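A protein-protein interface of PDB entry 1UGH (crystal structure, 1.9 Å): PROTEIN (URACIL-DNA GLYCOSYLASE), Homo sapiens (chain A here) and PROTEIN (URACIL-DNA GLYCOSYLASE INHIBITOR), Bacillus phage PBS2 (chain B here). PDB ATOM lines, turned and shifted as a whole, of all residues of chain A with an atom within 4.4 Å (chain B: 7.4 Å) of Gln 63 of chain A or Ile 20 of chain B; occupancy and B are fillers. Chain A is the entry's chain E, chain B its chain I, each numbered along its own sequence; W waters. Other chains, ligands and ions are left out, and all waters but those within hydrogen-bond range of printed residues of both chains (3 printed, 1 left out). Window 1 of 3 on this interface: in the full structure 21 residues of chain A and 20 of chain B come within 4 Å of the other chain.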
ATOM      1  N   GLY A  62     -19.427  17.827   2.768  1.00  0.00           N
ATOM      2  CA  GLY A  62     -19.264  16.696   1.884  1.00  0.00           C
ATOM      3  C   GLY A  62     -20.608  16.335   1.279  1.00  0.00           C
ATOM      4  O   GLY A  62     -21.560  17.134   1.316  1.00  0.00           O
ATOM      5  N   GLN A  63     -20.689  15.121   0.742  1.00  0.00           N
ATOM      6  CA  GLN A  63     -21.893  14.614   0.103  1.00  0.00           C
ATOM      7  C   GLN A  63     -22.456  13.459   0.929  1.00  0.00           C
ATOM      8  O   GLN A  63     -22.896  13.685   2.055  1.00  0.00           O
ATOM      9  CB  GLN A  63     -21.577  14.205  -1.334  1.00  0.00           C
ATOM     10  CG  GLN A  63     -21.084  15.382  -2.177  1.00  0.00           C
ATOM     11  CD  GLN A  63     -20.488  14.969  -3.513  1.00  0.00           C
ATOM     12  OE1 GLN A  63     -20.298  13.785  -3.782  1.00  0.00           O
ATOM     13  NE2 GLN A  63     -20.183  15.954  -4.356  1.00  0.00           N
ATOM     14  N   ASP A  64     -22.450  12.238   0.403  1.00  0.00           N
ATOM     15  CA  ASP A  64     -22.965  11.110   1.172  1.00  0.00           C
ATOM     16  C   ASP A  64     -21.793  10.306   1.718  1.00  0.00           C
ATOM     17  O   ASP A  64     -20.642  10.567   1.355  1.00  0.00           O
ATOM     18  CB  ASP A  64     -23.962  10.262   0.349  1.00  0.00           C
ATOM     19  CG  ASP A  64     -23.291   9.354  -0.679  1.00  0.00           C
ATOM     20  OD1 ASP A  64     -22.300   9.762  -1.320  1.00  0.00           O
ATOM     21  OD2 ASP A  64     -23.790   8.224  -0.873  1.00  0.00           O
ATOM     22  N   SER A  88      -9.542  11.166  -2.997  1.00  0.00           N
ATOM     23  CA  SER A  88      -9.773  12.548  -2.579  1.00  0.00           C
ATOM     24  C   SER A  88      -8.977  12.953  -1.335  1.00  0.00           C
ATOM     25  O   SER A  88      -8.334  14.000  -1.324  1.00  0.00           O
ATOM     26  CB  SER A  88     -11.264  12.818  -2.332  1.00  0.00           C
ATOM     27  OG  SER A  88     -11.963  13.007  -3.548  1.00  0.00           O
ATOM     28  N   ASN A 123     -21.440  15.942   6.171  1.00  0.00           N
ATOM     29  CA  ASN A 123     -21.923  15.394   4.899  1.00  0.00           C
ATOM     30  C   ASN A 123     -23.359  15.881   4.715  1.00  0.00           C
ATOM     31  O   ASN A 123     -24.066  16.107   5.706  1.00  0.00           O
ATOM     32  CB  ASN A 123     -21.953  13.865   4.925  1.00  0.00           C
ATOM     33  CG  ASN A 123     -20.717  13.252   4.342  1.00  0.00           C
ATOM     34  OD1 ASN A 123     -20.175  13.737   3.352  1.00  0.00           O
ATOM     35  ND2 ASN A 123     -20.254  12.184   4.950  1.00  0.00           N
ATOM     36  N   ALA A 124     -23.792  16.033   3.463  1.00  0.00           N
ATOM     37  CA  ALA A 124     -25.155  16.483   3.153  1.00  0.00           C
ATOM     38  C   ALA A 124     -26.189  15.376   3.426  1.00  0.00           C
ATOM     39  O   ALA A 124     -27.289  15.646   3.920  1.00  0.00           O
ATOM     40  CB  ALA A 124     -25.245  16.949   1.706  1.00  0.00           C
ATOM     41  N   VAL A 125     -25.818  14.138   3.106  1.00  0.00           N
ATOM     42  CA  VAL A 125     -26.666  12.977   3.316  1.00  0.00           C
ATOM     43  C   VAL A 125     -25.889  12.151   4.322  1.00  0.00           C
ATOM     44  O   VAL A 125     -24.755  11.782   4.055  1.00  0.00           O
ATOM     45  CB  VAL A 125     -26.838  12.192   2.008  1.00  0.00           C
ATOM     46  CG1 VAL A 125     -27.670  10.936   2.235  1.00  0.00           C
ATOM     47  CG2 VAL A 125     -27.485  13.081   0.960  1.00  0.00           C
ATOM     48  N   TYR A 167     -21.335  20.819  -5.988  1.00  0.00           N
ATOM     49  CA  TYR A 167     -22.378  20.345  -5.093  1.00  0.00           C
ATOM     50  C   TYR A 167     -22.262  21.090  -3.751  1.00  0.00           C
ATOM     51  O   TYR A 167     -23.212  21.735  -3.295  1.00  0.00           O
ATOM     52  CB  TYR A 167     -22.269  18.824  -4.872  1.00  0.00           C
ATOM     53  CG  TYR A 167     -23.316  18.276  -3.914  1.00  0.00           C
ATOM     54  CD1 TYR A 167     -23.104  18.290  -2.528  1.00  0.00           C
ATOM     55  CD2 TYR A 167     -24.557  17.831  -4.384  1.00  0.00           C
ATOM     56  CE1 TYR A 167     -24.098  17.896  -1.634  1.00  0.00           C
ATOM     57  CE2 TYR A 167     -25.566  17.426  -3.491  1.00  0.00           C
ATOM     58  CZ  TYR A 167     -25.330  17.468  -2.113  1.00  0.00           C
ATOM     59  OH  TYR A 167     -26.325  17.117  -1.218  1.00  0.00           O
ATOM     60  N   HIS A 187     -13.148  20.259  -6.527  1.00  0.00           N
ATOM     61  CA  HIS A 187     -13.157  19.119  -5.598  1.00  0.00           C
ATOM     62  C   HIS A 187     -11.795  18.398  -5.653  1.00  0.00           C
ATOM     63  O   HIS A 187     -11.199  18.295  -6.730  1.00  0.00           O
ATOM     64  CB  HIS A 187     -14.286  18.152  -5.996  1.00  0.00           C
ATOM     65  CG  HIS A 187     -14.566  17.072  -4.995  1.00  0.00           C
ATOM     66  ND1 HIS A 187     -13.854  15.891  -4.944  1.00  0.00           N
ATOM     67  CD2 HIS A 187     -15.494  16.987  -4.009  1.00  0.00           C
ATOM     68  CE1 HIS A 187     -14.325  15.127  -3.972  1.00  0.00           C
ATOM     69  NE2 HIS A 187     -15.323  15.769  -3.390  1.00  0.00           N
ATOM     70  N   SER A 189     -11.030  15.437  -5.892  1.00  0.00           N
ATOM     71  CA  SER A 189     -11.074  14.189  -6.632  1.00  0.00           C
ATOM     72  C   SER A 189     -10.065  14.269  -7.774  1.00  0.00           C
ATOM     73  O   SER A 189      -9.876  15.334  -8.361  1.00  0.00           O
ATOM     74  CB  SER A 189     -12.476  13.985  -7.219  1.00  0.00           C
ATOM     75  OG  SER A 189     -12.484  13.041  -8.279  1.00  0.00           O
ATOM     76  N   GLU B  18     -14.339   5.551  -3.560  1.00  0.00           N
ATOM     77  CA  GLU B  18     -15.246   6.684  -3.409  1.00  0.00           C
ATOM     78  C   GLU B  18     -16.032   6.939  -4.703  1.00  0.00           C
ATOM     79  O   GLU B  18     -15.664   6.437  -5.776  1.00  0.00           O
ATOM     80  CB  GLU B  18     -14.417   7.930  -3.071  1.00  0.00           C
ATOM     81  CG  GLU B  18     -13.351   8.218  -4.130  1.00  0.00           C
ATOM     82  CD  GLU B  18     -12.449   9.382  -3.799  1.00  0.00           C
ATOM     83  OE1 GLU B  18     -11.970   9.469  -2.655  1.00  0.00           O
ATOM     84  OE2 GLU B  18     -12.186  10.205  -4.690  1.00  0.00           O
ATOM     85  N   SER B  19     -17.136   7.672  -4.578  1.00  0.00           N
ATOM     86  CA  SER B  19     -17.984   8.057  -5.706  1.00  0.00           C
ATOM     87  C   SER B  19     -18.370   9.498  -5.414  1.00  0.00           C
ATOM     88  O   SER B  19     -19.067   9.774  -4.437  1.00  0.00           O
ATOM     89  CB  SER B  19     -19.237   7.185  -5.789  1.00  0.00           C
ATOM     90  OG  SER B  19     -18.895   5.816  -5.894  1.00  0.00           O
ATOM     91  N   ILE B  20     -17.847  10.411  -6.220  1.00  0.00           N
ATOM     92  CA  ILE B  20     -18.090  11.830  -6.035  1.00  0.00           C
ATOM     93  C   ILE B  20     -19.044  12.378  -7.090  1.00  0.00           C
ATOM     94  O   ILE B  20     -18.795  12.255  -8.283  1.00  0.00           O
ATOM     95  CB  ILE B  20     -16.750  12.619  -6.097  1.00  0.00           C
ATOM     96  CG1 ILE B  20     -15.729  12.035  -5.109  1.00  0.00           C
ATOM     97  CG2 ILE B  20     -16.992  14.095  -5.839  1.00  0.00           C
ATOM     98  CD1 ILE B  20     -16.133  12.109  -3.642  1.00  0.00           C
ATOM     99  N   LEU B  21     -20.138  12.981  -6.640  1.00  0.00           N
ATOM    100  CA  LEU B  21     -21.131  13.560  -7.538  1.00  0.00           C
ATOM    101  C   LEU B  21     -20.660  14.913  -8.064  1.00  0.00           C
ATOM    102  O   LEU B  21     -20.223  15.771  -7.291  1.00  0.00           O
ATOM    103  CB  LEU B  21     -22.454  13.736  -6.796  1.00  0.00           C
ATOM    104  CG  LEU B  21     -23.515  14.595  -7.488  1.00  0.00           C
ATOM    105  CD1 LEU B  21     -24.038  13.898  -8.726  1.00  0.00           C
ATOM    106  CD2 LEU B  21     -24.647  14.870  -6.521  1.00  0.00           C
ATOM    107  N   MET B  22     -20.782  15.116  -9.370  1.00  0.00           N
ATOM    108  CA  MET B  22     -20.375  16.373  -9.985  1.00  0.00           C
ATOM    109  C   MET B  22     -21.406  16.833 -11.003  1.00  0.00           C
ATOM    110  O   MET B  22     -22.098  16.020 -11.610  1.00  0.00           O
ATOM    111  CB  MET B  22     -18.986  16.249 -10.623  1.00  0.00           C
ATOM    112  CG  MET B  22     -17.837  16.352  -9.616  1.00  0.00           C
ATOM    113  SD  MET B  22     -16.200  16.315 -10.368  1.00  0.00           S
ATOM    114  CE  MET B  22     -15.383  15.098  -9.347  1.00  0.00           C
ATOM    115  N   LEU B  23     -21.504  18.146 -11.172  1.00  0.00           N
ATOM    116  CA  LEU B  23     -22.452  18.760 -12.091  1.00  0.00           C
ATOM    117  C   LEU B  23     -21.942  18.714 -13.515  1.00  0.00           C
ATOM    118  O   LEU B  23     -20.759  18.898 -13.752  1.00  0.00           O
ATOM    119  CB  LEU B  23     -22.725  20.208 -11.672  1.00  0.00           C
ATOM    120  CG  LEU B  23     -23.757  20.404 -10.552  1.00  0.00           C
ATOM    121  CD1 LEU B  23     -23.315  19.758  -9.246  1.00  0.00           C
ATOM    122  CD2 LEU B  23     -23.986  21.872 -10.349  1.00  0.00           C
ATOM    123  N   GLU B  26     -19.300  21.078 -14.635  1.00  0.00           N
ATOM    124  CA  GLU B  26     -18.133  20.880 -13.783  1.00  0.00           C
ATOM    125  C   GLU B  26     -17.324  19.784 -14.473  1.00  0.00           C
ATOM    126  O   GLU B  26     -16.097  19.867 -14.586  1.00  0.00           O
ATOM    127  CB  GLU B  26     -18.606  20.426 -12.399  1.00  0.00           C
ATOM    128  CG  GLU B  26     -17.533  20.221 -11.352  1.00  0.00           C
ATOM    129  CD  GLU B  26     -18.120  19.955  -9.976  1.00  0.00           C
ATOM    130  OE1 GLU B  26     -19.332  19.684  -9.877  1.00  0.00           O
ATOM    131  OE2 GLU B  26     -17.370  20.027  -8.986  1.00  0.00           O
ATOM    132  N   VAL B  27     -18.050  18.787 -14.974  1.00  0.00           N
ATOM    133  CA  VAL B  27     -17.496  17.646 -15.698  1.00  0.00           C
ATOM    134  C   VAL B  27     -17.047  18.062 -17.107  1.00  0.00           C
ATOM    135  O   VAL B  27     -15.990  17.655 -17.577  1.00  0.00           O
ATOM    136  CB  VAL B  27     -18.547  16.499 -15.812  1.00  0.00           C
ATOM    137  CG1 VAL B  27     -18.085  15.449 -16.787  1.00  0.00           C
ATOM    138  CG2 VAL B  27     -18.793  15.861 -14.457  1.00  0.00           C
ATOM    139  N   ASP B  38     -26.040  14.774 -14.013  1.00  0.00           N
ATOM    140  CA  ASP B  38     -25.050  14.776 -12.941  1.00  0.00           C
ATOM    141  C   ASP B  38     -24.239  13.493 -12.986  1.00  0.00           C
ATOM    142  O   ASP B  38     -24.794  12.387 -13.032  1.00  0.00           O
ATOM    143  CB  ASP B  38     -25.731  14.895 -11.578  1.00  0.00           C
ATOM    144  CG  ASP B  38     -26.167  16.313 -11.258  1.00  0.00           C
ATOM    145  OD1 ASP B  38     -26.025  17.206 -12.118  1.00  0.00           O
ATOM    146  OD2 ASP B  38     -26.651  16.535 -10.130  1.00  0.00           O
ATOM    147  N   ILE B  39     -22.922  13.646 -12.931  1.00  0.00           N
ATOM    148  CA  ILE B  39     -22.017  12.512 -13.001  1.00  0.00           C
ATOM    149  C   ILE B  39     -21.438  12.066 -11.666  1.00  0.00           C
ATOM    150  O   ILE B  39     -20.963  12.881 -10.869  1.00  0.00           O
ATOM    151  CB  ILE B  39     -20.846  12.789 -13.965  1.00  0.00           C
ATOM    152  CG1 ILE B  39     -21.374  12.985 -15.391  1.00  0.00           C
ATOM    153  CG2 ILE B  39     -19.831  11.652 -13.905  1.00  0.00           C
ATOM    154  CD1 ILE B  39     -22.127  11.786 -15.962  1.00  0.00           C
ATOM    155  N   LEU B  40     -21.470  10.758 -11.446  1.00  0.00           N
ATOM    156  CA  LEU B  40     -20.924  10.163 -10.245  1.00  0.00           C
ATOM    157  C   LEU B  40     -19.567   9.618 -10.658  1.00  0.00           C
ATOM    158  O   LEU B  40     -19.478   8.727 -11.505  1.00  0.00           O
ATOM    159  CB  LEU B  40     -21.816   9.025  -9.735  1.00  0.00           C
ATOM    160  CG  LEU B  40     -22.949   9.379  -8.770  1.00  0.00           C
ATOM    161  CD1 LEU B  40     -23.913   8.219  -8.653  1.00  0.00           C
ATOM    162  CD2 LEU B  40     -22.378   9.731  -7.410  1.00  0.00           C
ATOM    163  N   VAL B  41     -18.513  10.208 -10.111  1.00  0.00           N
ATOM    164  CA  VAL B  41     -17.157   9.796 -10.412  1.00  0.00           C
ATOM    165  C   VAL B  41     -16.720   8.714  -9.438  1.00  0.00           C
ATOM    166  O   VAL B  41     -16.274   8.994  -8.328  1.00  0.00           O
ATOM    167  CB  VAL B  41     -16.184  10.981 -10.348  1.00  0.00           C
ATOM    168  CG1 VAL B  41     -14.839  10.591 -10.958  1.00  0.00           C
ATOM    169  CG2 VAL B  41     -16.773  12.174 -11.066  1.00  0.00           C
ATOM    170  N   HIS B  42     -16.892   7.472  -9.860  1.00  0.00           N
ATOM    171  CA  HIS B  42     -16.519   6.314  -9.062  1.00  0.00           C
ATOM    172  C   HIS B  42     -15.022   6.113  -9.271  1.00  0.00           C
ATOM    173  O   HIS B  42     -14.588   5.770 -10.370  1.00  0.00           O
ATOM    174  CB  HIS B  42     -17.286   5.081  -9.551  1.00  0.00           C
ATOM    175  CG  HIS B  42     -18.768   5.264  -9.564  1.00  0.00           C
ATOM    176  ND1 HIS B  42     -19.436   5.861 -10.611  1.00  0.00           N
ATOM    177  CD2 HIS B  42     -19.711   4.952  -8.646  1.00  0.00           C
ATOM    178  CE1 HIS B  42     -20.729   5.912 -10.334  1.00  0.00           C
ATOM    179  NE2 HIS B  42     -20.920   5.366  -9.148  1.00  0.00           N
ATOM    180  N   THR B  43     -14.241   6.310  -8.214  1.00  0.00           N
ATOM    181  CA  THR B  43     -12.792   6.199  -8.299  1.00  0.00           C
ATOM    182  C   THR B  43     -12.195   5.048  -7.503  1.00  0.00           C
ATOM    183  O   THR B  43     -12.560   4.810  -6.350  1.00  0.00           O
ATOM    184  CB  THR B  43     -12.132   7.503  -7.806  1.00  0.00           C
ATOM    185  OG1 THR B  43     -12.843   8.625  -8.344  1.00  0.00           O
ATOM    186  CG2 THR B  43     -10.673   7.571  -8.248  1.00  0.00           C
ATOM    187  N   LEU B  56     -17.197   6.945 -14.699  1.00  0.00           N
ATOM    188  CA  LEU B  56     -18.189   8.016 -14.600  1.00  0.00           C
ATOM    189  C   LEU B  56     -19.565   7.530 -15.081  1.00  0.00           C
ATOM    190  O   LEU B  56     -19.739   7.127 -16.238  1.00  0.00           O
ATOM    191  CB  LEU B  56     -17.756   9.234 -15.433  1.00  0.00           C
ATOM    192  CG  LEU B  56     -16.649  10.187 -14.966  1.00  0.00           C
ATOM    193  CD1 LEU B  56     -15.369   9.460 -14.635  1.00  0.00           C
ATOM    194  CD2 LEU B  56     -16.395  11.213 -16.052  1.00  0.00           C
ATOM    195  N   THR B  57     -20.549   7.553 -14.195  1.00  0.00           N
ATOM    196  CA  THR B  57     -21.875   7.114 -14.585  1.00  0.00           C
ATOM    197  C   THR B  57     -22.838   8.256 -14.320  1.00  0.00           C
ATOM    198  O   THR B  57     -22.418   9.369 -13.972  1.00  0.00           O
ATOM    199  CB  THR B  57     -22.325   5.869 -13.786  1.00  0.00           C
ATOM    200  OG1 THR B  57     -22.660   6.245 -12.447  1.00  0.00           O
ATOM    201  CG2 THR B  57     -21.228   4.820 -13.760  1.00  0.00           C
HETATM  202  O   HOH W   1     -19.406  18.575  -6.963  1.00  0.00           O
HETATM  203  O   HOH W   2     -13.309  10.806  -6.956  1.00  0.00           O
HETATM  204  O   HOH W   3     -14.742  20.086  -9.053  1.00  0.00           O
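The side-chain amide nitrogen (NE2) of Gln 63 of chain A lies within hydrogen-bond range of the backbone carbonyl oxygen (O) of Leu 21 of chain B. OE1 of Glu 18 of chain B sits at hydrogen-bond distance from N of Ser 88 of chain A.
N of Gln 63 of chain A is in hydrogen-bond range of OD1 of Asn 123 of chain A, at 3.0 Å. The backbone NH (N) of Ala 124 of chain A is in hydrogen-bond range of the backbone carbonyl oxygen (O) of Gln 63 of chain A (2.9 Å). The backbone carbonyl oxygen (O) of Gln 63 of chain A lies within hydrogen-bond range of the backbone NH (N) of Val 125 of chain A (3.1 Å). ND1 of His 187 of chain A is in hydrogen-bond range of N of Ser 189 of chain A (3.0 Å). O of Ile 20 of chain B sits at hydrogen-bond distance from N of Val 41 of chain B, 2.8 Å away. N of Met 22 of chain B is in hydrogen-bond range of O of Ile 39 of chain B (2.7 Å).
Gln 63 of chain A touches Ile 20 of chain B. Leu 21 of chain B touches Tyr 167 of chain A (CD2 to CD2, 3.7 Å). Tyr 167 of chain A touches Leu 23 of chain B. Ile 20 of chain B touches His 187 of chain A. Met 22 of chain B touches Ser 189 of chain A (CE to OG, 3.7 Å).
Gly 62 of chain A touches none of the printed residues of chain B. Of chain B, only Ile 20 and Leu 21 come within 4 Å of Gln 63 of chain A. Of the printed residues of chain B, Ser 88 of chain A touches Glu 18. Printed residues of chain B within 4 Å of Tyr 167 of chain A: Leu 21 (3.7 Å) and Leu 23 (3.96 Å). Of the printed residues of chain A, Glu 18 of chain B touches Ser 88 (3.0 Å). Ile 20 of chain B touches just these residues of chain A: Gln 63 (3.7 Å) and His 187 (3.4 Å). Of the printed residues of chain A, Met 22 of chain B touches Ser 189. The nearest residue of chain A that does not touch Ile 20 of chain B is Ser 88 of chain A (4.2 Å). The nearest printed residue of chain B that does not touch Ser 189 of chain A is Val 41 of chain B (4.3 Å).
Of the 10 printed residues of chain A, 5 touch a printed residue of chain B. Printed residues of chain A that touch a printed residue of chain B: Gln 63, Ser 88, Tyr 167, His 187 and Ser 189. Hydrophobic or aromatic side chains of chain A that line the printed part of chain B: Tyr 167 and His 187. Hydrophobic or aromatic side chains of chain B that line the printed part of chain A: Ile 20, Leu 21, Met 22 and Leu 23. Among the printed residues, 7 pairs touch across the chains. Among the printed residues, no Asp or Glu carboxylate lies within 4 Å of a Lys or Arg side-chain nitrogen of the other chain.
Water W2 lies within hydrogen-bond range of OE2 of Glu 18 of chain B (2.6 Å), OG1 of Thr 43 of chain B (2.6 Å) and OG of Ser 189 of chain A (2.7 Å). Water W3 bridges OE2 of Glu 26 of chain B (2.6 Å) and N of His 187 of chain A (3.0 Å). Water W1 lies within hydrogen-bond range of the backbone carbonyl oxygen (O) of Leu 21 of chain B, the backbone NH (N) of Tyr 167 of chain A and the side-chain carboxylate (OE1) of Glu 26 of chain B.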
